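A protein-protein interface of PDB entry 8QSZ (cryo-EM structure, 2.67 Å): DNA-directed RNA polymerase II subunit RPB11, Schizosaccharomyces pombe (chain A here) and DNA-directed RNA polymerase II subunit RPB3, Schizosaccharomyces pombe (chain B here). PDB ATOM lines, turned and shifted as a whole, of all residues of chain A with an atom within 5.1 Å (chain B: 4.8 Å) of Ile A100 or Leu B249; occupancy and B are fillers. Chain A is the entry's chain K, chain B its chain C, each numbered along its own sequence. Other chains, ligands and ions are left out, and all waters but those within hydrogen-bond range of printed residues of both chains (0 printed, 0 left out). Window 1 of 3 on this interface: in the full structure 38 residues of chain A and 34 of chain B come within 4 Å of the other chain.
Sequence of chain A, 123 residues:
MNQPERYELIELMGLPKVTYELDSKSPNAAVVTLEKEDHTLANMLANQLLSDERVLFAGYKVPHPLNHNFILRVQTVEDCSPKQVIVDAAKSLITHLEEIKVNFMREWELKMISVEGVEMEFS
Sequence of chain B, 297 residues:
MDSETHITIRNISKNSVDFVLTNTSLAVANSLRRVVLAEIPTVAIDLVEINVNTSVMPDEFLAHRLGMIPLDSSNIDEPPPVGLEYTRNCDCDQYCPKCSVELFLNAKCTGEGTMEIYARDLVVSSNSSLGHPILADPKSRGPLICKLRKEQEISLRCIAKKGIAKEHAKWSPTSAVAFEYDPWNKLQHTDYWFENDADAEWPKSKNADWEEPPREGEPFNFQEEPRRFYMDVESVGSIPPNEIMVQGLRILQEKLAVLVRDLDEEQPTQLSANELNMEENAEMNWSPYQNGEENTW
OE1 of Gln B253 is in hydrogen-bond range of NZ of Lys A101.
The backbone carbonyl oxygen (O) of Leu B249 sits close to the side-chain amide oxygen (OE1) of Gln B253 (3.4 Å). OE1 of Gln B247 sits at hydrogen-bond distance from NH1 of Arg B250, 2.4 Å away. N of His A96 lies close to OE1 of Glu A99.
Among the printed residues, pairs that only touch across the chains: His A96 with Thr B5 (2.8 Å), His A96 with Thr B24 (3.7 Å), Leu A97 with Leu B249 (3.9 Å), Leu A97 with Leu B252 (3.8 Å), Leu A97 with Gln B253 (3.7 Å), Glu A98 with Gln B253 (3.6 Å), Glu A99 with Thr B5 (3.4 Å), Ile A100 with Thr B5 (3.3 Å), Ile A100 with Ile B7 (3.6 Å), Ile A100 with Leu B21 (3.9 Å), Ile A100 with Thr B24 (3.6 Å), Ile A100 with Leu B249 (3.5 Å), Lys A101 with Leu B249 (3.7 Å), Lys A101 with Arg B250 (3.3 Å), Asn A103 with Thr B5 (3.7 Å), Asn A103 with Ile B7 (3.7 Å), Phe A104 with Ile B7 (3.5 Å), Phe A104 with Met B245 (3.5 Å) and Met A105 with Val B246 (3.8 Å).
Of chain B, only Thr B5 (3.3 Å), Ile B7 (3.6 Å), Leu B21 (3.9 Å), Thr B24 (3.6 Å) and Leu B249 (3.5 Å) come within 4 Å of Ile A100. Of the printed residues of chain B, Lys A101 touches Leu B249, Arg B250 and Gln B253. Val A102 touches none of the printed residues of chain B. Of the printed residues of chain B, Asn A103 touches Thr B5 (3.7 Å) and Ile B7 (3.7 Å). Printed residues of chain B within 4 Å of Phe A104: Ile B7 (3.5 Å) and Met B245 (3.5 Å). Leu B32 touches none of the printed residues of chain A. Printed residues of chain A within 4 Å of Met B245: Phe A104 (3.5 Å). Leu B249 touches just these residues of chain A: Leu A97 (3.9 Å), Ile A100 (3.5 Å) and Lys A101 (3.7 Å). Of the printed residues of chain A, Leu B252 touches Leu A97. The nearest printed residue of chain B that does not touch Ile A100 is Leu B32 (5.1 Å). The nearest residue of chain A that does not touch Leu B249 is Phe A104 (4.9 Å). The nearest printed residue of chain B that does not touch Asn A103 is Leu B249 (7.5 Å).
Of the 14 printed residues of chain B, 10 touch a printed residue of chain A. Hydrophobic or aromatic side chains of chain B that line the printed part of chain A: Ile B7, Leu B21, Met B245, Val B246, Leu B249 and Leu B252.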
ATOM      1  N   HIS A  96      16.808  17.266  27.114  1.00  0.00           N
ATOM      2  CA  HIS A  96      17.566  17.729  25.955  1.00  0.00           C
ATOM      3  C   HIS A  96      18.852  16.936  25.790  1.00  0.00           C
ATOM      4  O   HIS A  96      19.171  16.459  24.695  1.00  0.00           O
ATOM      5  CB  HIS A  96      17.878  19.215  26.112  1.00  0.00           C
ATOM      6  CG  HIS A  96      18.178  19.915  24.826  1.00  0.00           C
ATOM      7  ND1 HIS A  96      19.399  20.499  24.565  1.00  0.00           N
ATOM      8  CD2 HIS A  96      17.416  20.133  23.731  1.00  0.00           C
ATOM      9  CE1 HIS A  96      19.377  21.041  23.362  1.00  0.00           C
ATOM     10  NE2 HIS A  96      18.182  20.837  22.837  1.00  0.00           N
ATOM     11  N   LEU A  97      19.610  16.795  26.876  1.00  0.00           N
ATOM     12  CA  LEU A  97      20.837  16.017  26.824  1.00  0.00           C
ATOM     13  C   LEU A  97      20.540  14.583  26.421  1.00  0.00           C
ATOM     14  O   LEU A  97      21.354  13.939  25.755  1.00  0.00           O
ATOM     15  CB  LEU A  97      21.541  16.066  28.178  1.00  0.00           C
ATOM     16  CG  LEU A  97      21.959  17.463  28.639  1.00  0.00           C
ATOM     17  CD1 LEU A  97      22.185  17.469  30.129  1.00  0.00           C
ATOM     18  CD2 LEU A  97      23.195  17.950  27.903  1.00  0.00           C
ATOM     19  N   GLU A  98      19.376  14.063  26.818  1.00  0.00           N
ATOM     20  CA  GLU A  98      19.024  12.700  26.434  1.00  0.00           C
ATOM     21  C   GLU A  98      18.822  12.570  24.926  1.00  0.00           C
ATOM     22  O   GLU A  98      19.279  11.591  24.324  1.00  0.00           O
ATOM     23  CB  GLU A  98      17.777  12.249  27.188  1.00  0.00           C
ATOM     24  CG  GLU A  98      17.378  10.821  26.896  1.00  0.00           C
ATOM     25  CD  GLU A  98      18.481   9.835  27.219  1.00  0.00           C
ATOM     26  OE1 GLU A  98      18.624   9.460  28.401  1.00  0.00           O
ATOM     27  OE2 GLU A  98      19.219   9.444  26.293  1.00  0.00           O
ATOM     28  N   GLU A  99      18.134  13.527  24.285  1.00  0.00           N
ATOM     29  CA  GLU A  99      18.084  13.464  22.818  1.00  0.00           C
ATOM     30  C   GLU A  99      19.467  13.636  22.203  1.00  0.00           C
ATOM     31  O   GLU A  99      19.789  12.973  21.211  1.00  0.00           O
ATOM     32  CB  GLU A  99      17.123  14.463  22.153  1.00  0.00           C
ATOM     33  CG  GLU A  99      15.611  14.265  22.362  1.00  0.00           C
ATOM     34  CD  GLU A  99      15.064  14.854  23.641  1.00  0.00           C
ATOM     35  OE1 GLU A  99      15.838  15.500  24.357  1.00  0.00           O
ATOM     36  OE2 GLU A  99      13.868  14.647  23.943  1.00  0.00           O
ATOM     37  N   ILE A 100      20.288  14.535  22.746  1.00  0.00           N
ATOM     38  CA  ILE A 100      21.651  14.666  22.230  1.00  0.00           C
ATOM     39  C   ILE A 100      22.337  13.307  22.244  1.00  0.00           C
ATOM     40  O   ILE A 100      22.929  12.873  21.251  1.00  0.00           O
ATOM     41  CB  ILE A 100      22.451  15.697  23.052  1.00  0.00           C
ATOM     42  CG1 ILE A 100      21.801  17.081  23.033  1.00  0.00           C
ATOM     43  CG2 ILE A 100      23.859  15.807  22.518  1.00  0.00           C
ATOM     44  CD1 ILE A 100      21.692  17.691  21.677  1.00  0.00           C
ATOM     45  N   LYS A 101      22.232  12.608  23.373  1.00  0.00           N
ATOM     46  CA  LYS A 101      22.873  11.310  23.546  1.00  0.00           C
ATOM     47  C   LYS A 101      22.347  10.294  22.544  1.00  0.00           C
ATOM     48  O   LYS A 101      23.120   9.614  21.859  1.00  0.00           O
ATOM     49  CB  LYS A 101      22.603  10.821  24.964  1.00  0.00           C
ATOM     50  CG  LYS A 101      23.313   9.563  25.382  1.00  0.00           C
ATOM     51  CD  LYS A 101      22.819   9.159  26.752  1.00  0.00           C
ATOM     52  CE  LYS A 101      23.321  10.083  27.828  1.00  0.00           C
ATOM     53  NZ  LYS A 101      22.884   9.612  29.165  1.00  0.00           N
ATOM     54  N   VAL A 102      21.023  10.163  22.466  1.00  0.00           N
ATOM     55  CA  VAL A 102      20.420   9.147  21.612  1.00  0.00           C
ATOM     56  C   VAL A 102      20.796   9.390  20.160  1.00  0.00           C
ATOM     57  O   VAL A 102      21.163   8.463  19.427  1.00  0.00           O
ATOM     58  CB  VAL A 102      18.893   9.132  21.801  1.00  0.00           C
ATOM     59  CG1 VAL A 102      18.240   8.248  20.760  1.00  0.00           C
ATOM     60  CG2 VAL A 102      18.540   8.665  23.198  1.00  0.00           C
ATOM     61  N   ASN A 103      20.707  10.643  19.718  1.00  0.00           N
ATOM     62  CA  ASN A 103      20.987  10.936  18.322  1.00  0.00           C
ATOM     63  C   ASN A 103      22.469  10.768  18.018  1.00  0.00           C
ATOM     64  O   ASN A 103      22.832  10.299  16.934  1.00  0.00           O
ATOM     65  CB  ASN A 103      20.506  12.341  17.980  1.00  0.00           C
ATOM     66  CG  ASN A 103      20.567  12.626  16.502  1.00  0.00           C
ATOM     67  OD1 ASN A 103      21.302  11.979  15.758  1.00  0.00           O
ATOM     68  ND2 ASN A 103      19.752  13.562  16.058  1.00  0.00           N
ATOM     69  N   PHE A 104      23.342  11.118  18.966  1.00  0.00           N
ATOM     70  CA  PHE A 104      24.765  10.870  18.771  1.00  0.00           C
ATOM     71  C   PHE A 104      25.035   9.386  18.601  1.00  0.00           C
ATOM     72  O   PHE A 104      25.783   8.982  17.708  1.00  0.00           O
ATOM     73  CB  PHE A 104      25.574  11.403  19.949  1.00  0.00           C
ATOM     74  CG  PHE A 104      27.044  11.130  19.829  1.00  0.00           C
ATOM     75  CD1 PHE A 104      27.820  11.836  18.923  1.00  0.00           C
ATOM     76  CD2 PHE A 104      27.645  10.149  20.595  1.00  0.00           C
ATOM     77  CE1 PHE A 104      29.167  11.579  18.801  1.00  0.00           C
ATOM     78  CE2 PHE A 104      28.988   9.887  20.474  1.00  0.00           C
ATOM     79  CZ  PHE A 104      29.751  10.602  19.578  1.00  0.00           C
ATOM     80  N   MET A 105      24.454   8.556  19.470  1.00  0.00           N
ATOM     81  CA  MET A 105      24.710   7.123  19.386  1.00  0.00           C
ATOM     82  C   MET A 105      24.187   6.550  18.076  1.00  0.00           C
ATOM     83  O   MET A 105      24.860   5.733  17.433  1.00  0.00           O
ATOM     84  CB  MET A 105      24.085   6.404  20.577  1.00  0.00           C
ATOM     85  CG  MET A 105      24.747   6.728  21.902  1.00  0.00           C
ATOM     86  SD  MET A 105      24.311   5.570  23.204  1.00  0.00           S
ATOM     87  CE  MET A 105      22.618   6.040  23.525  1.00  0.00           C
ATOM     88  N   THR B   5      16.821  18.066  18.784  1.00  0.00           N
ATOM     89  CA  THR B   5      18.235  18.310  18.526  1.00  0.00           C
ATOM     90  C   THR B   5      18.724  17.459  17.369  1.00  0.00           C
ATOM     91  O   THR B   5      17.945  16.727  16.761  1.00  0.00           O
ATOM     92  CB  THR B   5      19.084  18.003  19.743  1.00  0.00           C
ATOM     93  OG1 THR B   5      18.777  16.688  20.213  1.00  0.00           O
ATOM     94  CG2 THR B   5      18.797  18.991  20.824  1.00  0.00           C
ATOM     95  N   ILE B   7      22.706  15.704  15.544  1.00  0.00           N
ATOM     96  CA  ILE B   7      24.152  15.580  15.441  1.00  0.00           C
ATOM     97  C   ILE B   7      24.488  15.035  14.063  1.00  0.00           C
ATOM     98  O   ILE B   7      23.819  14.128  13.562  1.00  0.00           O
ATOM     99  CB  ILE B   7      24.727  14.689  16.560  1.00  0.00           C
ATOM    100  CG1 ILE B   7      24.834  15.513  17.841  1.00  0.00           C
ATOM    101  CG2 ILE B   7      26.074  14.121  16.157  1.00  0.00           C
ATOM    102  CD1 ILE B   7      25.109  14.727  19.072  1.00  0.00           C
ATOM    103  N   LEU B  21      26.995  19.857  16.052  1.00  0.00           N
ATOM    104  CA  LEU B  21      25.903  19.862  17.013  1.00  0.00           C
ATOM    105  C   LEU B  21      24.947  20.993  16.653  1.00  0.00           C
ATOM    106  O   LEU B  21      25.340  22.161  16.644  1.00  0.00           O
ATOM    107  CB  LEU B  21      26.452  20.033  18.428  1.00  0.00           C
ATOM    108  CG  LEU B  21      25.494  19.886  19.604  1.00  0.00           C
ATOM    109  CD1 LEU B  21      24.808  18.542  19.569  1.00  0.00           C
ATOM    110  CD2 LEU B  21      26.248  20.057  20.906  1.00  0.00           C
ATOM    111  N   THR B  24      20.914  23.385  19.403  1.00  0.00           N
ATOM    112  CA  THR B  24      21.337  23.428  20.791  1.00  0.00           C
ATOM    113  C   THR B  24      21.782  24.841  21.120  1.00  0.00           C
ATOM    114  O   THR B  24      22.206  25.593  20.242  1.00  0.00           O
ATOM    115  CB  THR B  24      22.482  22.440  21.065  1.00  0.00           C
ATOM    116  OG1 THR B  24      22.118  21.139  20.596  1.00  0.00           O
ATOM    117  CG2 THR B  24      22.782  22.361  22.543  1.00  0.00           C
ATOM    118  N   LEU B  32      29.145  20.718  27.447  1.00  0.00           N
ATOM    119  CA  LEU B  32      29.650  19.452  26.932  1.00  0.00           C
ATOM    120  C   LEU B  32      31.164  19.501  26.771  1.00  0.00           C
ATOM    121  O   LEU B  32      31.878  18.580  27.180  1.00  0.00           O
ATOM    122  CB  LEU B  32      28.972  19.133  25.602  1.00  0.00           C
ATOM    123  CG  LEU B  32      29.295  17.798  24.935  1.00  0.00           C
ATOM    124  CD1 LEU B  32      29.081  16.640  25.886  1.00  0.00           C
ATOM    125  CD2 LEU B  32      28.450  17.632  23.689  1.00  0.00           C
ATOM    126  N   MET B 245      32.026  11.142  24.494  1.00  0.00           N
ATOM    127  CA  MET B 245      30.849  11.974  24.269  1.00  0.00           C
ATOM    128  C   MET B 245      29.666  11.485  25.097  1.00  0.00           C
ATOM    129  O   MET B 245      28.995  12.269  25.784  1.00  0.00           O
ATOM    130  CB  MET B 245      30.507  11.967  22.781  1.00  0.00           C
ATOM    131  CG  MET B 245      31.443  12.811  21.929  1.00  0.00           C
ATOM    132  SD  MET B 245      31.181  14.593  22.044  1.00  0.00           S
ATOM    133  CE  MET B 245      29.395  14.718  22.133  1.00  0.00           C
ATOM    134  N   VAL B 246      29.400  10.179  25.046  1.00  0.00           N
ATOM    135  CA  VAL B 246      28.261   9.626  25.771  1.00  0.00           C
ATOM    136  C   VAL B 246      28.431   9.833  27.268  1.00  0.00           C
ATOM    137  O   VAL B 246      27.477  10.179  27.972  1.00  0.00           O
ATOM    138  CB  VAL B 246      28.075   8.139  25.422  1.00  0.00           C
ATOM    139  CG1 VAL B 246      27.019   7.516  26.314  1.00  0.00           C
ATOM    140  CG2 VAL B 246      27.699   7.984  23.966  1.00  0.00           C
ATOM    141  N   GLN B 247      29.641   9.622  27.784  1.00  0.00           N
ATOM    142  CA  GLN B 247      29.906   9.828  29.199  1.00  0.00           C
ATOM    143  C   GLN B 247      29.775  11.281  29.623  1.00  0.00           C
ATOM    144  O   GLN B 247      29.289  11.544  30.725  1.00  0.00           O
ATOM    145  CB  GLN B 247      31.304   9.322  29.544  1.00  0.00           C
ATOM    146  CG  GLN B 247      31.349   7.845  29.853  1.00  0.00           C
ATOM    147  CD  GLN B 247      30.773   7.540  31.215  1.00  0.00           C
ATOM    148  OE1 GLN B 247      29.713   6.928  31.331  1.00  0.00           O
ATOM    149  NE2 GLN B 247      31.455   7.990  32.257  1.00  0.00           N
ATOM    150  N   GLY B 248      30.204  12.225  28.792  1.00  0.00           N
ATOM    151  CA  GLY B 248      30.017  13.624  29.112  1.00  0.00           C
ATOM    152  C   GLY B 248      28.547  13.968  29.202  1.00  0.00           C
ATOM    153  O   GLY B 248      28.109  14.664  30.128  1.00  0.00           O
ATOM    154  N   LEU B 249      27.772  13.475  28.234  1.00  0.00           N
ATOM    155  CA  LEU B 249      26.333  13.702  28.260  1.00  0.00           C
ATOM    156  C   LEU B 249      25.657  13.039  29.452  1.00  0.00           C
ATOM    157  O   LEU B 249      24.676  13.585  29.962  1.00  0.00           O
ATOM    158  CB  LEU B 249      25.702  13.208  26.960  1.00  0.00           C
ATOM    159  CG  LEU B 249      26.014  14.071  25.739  1.00  0.00           C
ATOM    160  CD1 LEU B 249      25.803  13.294  24.467  1.00  0.00           C
ATOM    161  CD2 LEU B 249      25.157  15.313  25.746  1.00  0.00           C
ATOM    162  N   ARG B 250      26.146  11.886  29.903  1.00  0.00           N
ATOM    163  CA  ARG B 250      25.642  11.279  31.128  1.00  0.00           C
ATOM    164  C   ARG B 250      26.007  12.078  32.366  1.00  0.00           C
ATOM    165  O   ARG B 250      25.187  12.202  33.280  1.00  0.00           O
ATOM    166  CB  ARG B 250      26.190   9.860  31.300  1.00  0.00           C
ATOM    167  CG  ARG B 250      25.942   8.931  30.141  1.00  0.00           C
ATOM    168  CD  ARG B 250      25.459   7.579  30.617  1.00  0.00           C
ATOM    169  NE  ARG B 250      25.646   6.544  29.607  1.00  0.00           N
ATOM    170  CZ  ARG B 250      26.731   5.790  29.493  1.00  0.00           C
ATOM    171  NH1 ARG B 250      27.767   5.938  30.301  1.00  0.00           N
ATOM    172  NH2 ARG B 250      26.779   4.865  28.539  1.00  0.00           N
ATOM    173  N   ILE B 251      27.224  12.613  32.420  1.00  0.00           N
ATOM    174  CA  ILE B 251      27.673  13.335  33.604  1.00  0.00           C
ATOM    175  C   ILE B 251      26.911  14.644  33.759  1.00  0.00           C
ATOM    176  O   ILE B 251      26.526  15.019  34.872  1.00  0.00           O
ATOM    177  CB  ILE B 251      29.193  13.560  33.529  1.00  0.00           C
ATOM    178  CG1 ILE B 251      29.926  12.241  33.769  1.00  0.00           C
ATOM    179  CG2 ILE B 251      29.633  14.599  34.545  1.00  0.00           C
ATOM    180  CD1 ILE B 251      31.300  12.190  33.166  1.00  0.00           C
ATOM    181  N   LEU B 252      26.681  15.360  32.655  1.00  0.00           N
ATOM    182  CA  LEU B 252      25.875  16.575  32.731  1.00  0.00           C
ATOM    183  C   LEU B 252      24.467  16.260  33.221  1.00  0.00           C
ATOM    184  O   LEU B 252      23.924  16.944  34.102  1.00  0.00           O
ATOM    185  CB  LEU B 252      25.822  17.254  31.365  1.00  0.00           C
ATOM    186  CG  LEU B 252      27.105  17.920  30.877  1.00  0.00           C
ATOM    187  CD1 LEU B 252      26.984  18.242  29.405  1.00  0.00           C
ATOM    188  CD2 LEU B 252      27.406  19.171  31.676  1.00  0.00           C
ATOM    189  N   GLN B 253      23.865  15.212  32.657  1.00  0.00           N
ATOM    190  CA  GLN B 253      22.542  14.783  33.090  1.00  0.00           C
ATOM    191  C   GLN B 253      22.524  14.476  34.577  1.00  0.00           C
ATOM    192  O   GLN B 253      21.579  14.840  35.278  1.00  0.00           O
ATOM    193  CB  GLN B 253      22.113  13.549  32.303  1.00  0.00           C
ATOM    194  CG  GLN B 253      21.198  13.828  31.145  1.00  0.00           C
ATOM    195  CD  GLN B 253      20.847  12.574  30.389  1.00  0.00           C
ATOM    196  OE1 GLN B 253      21.630  12.086  29.576  1.00  0.00           O
ATOM    197  NE2 GLN B 253      19.671  12.029  30.660  1.00  0.00           N
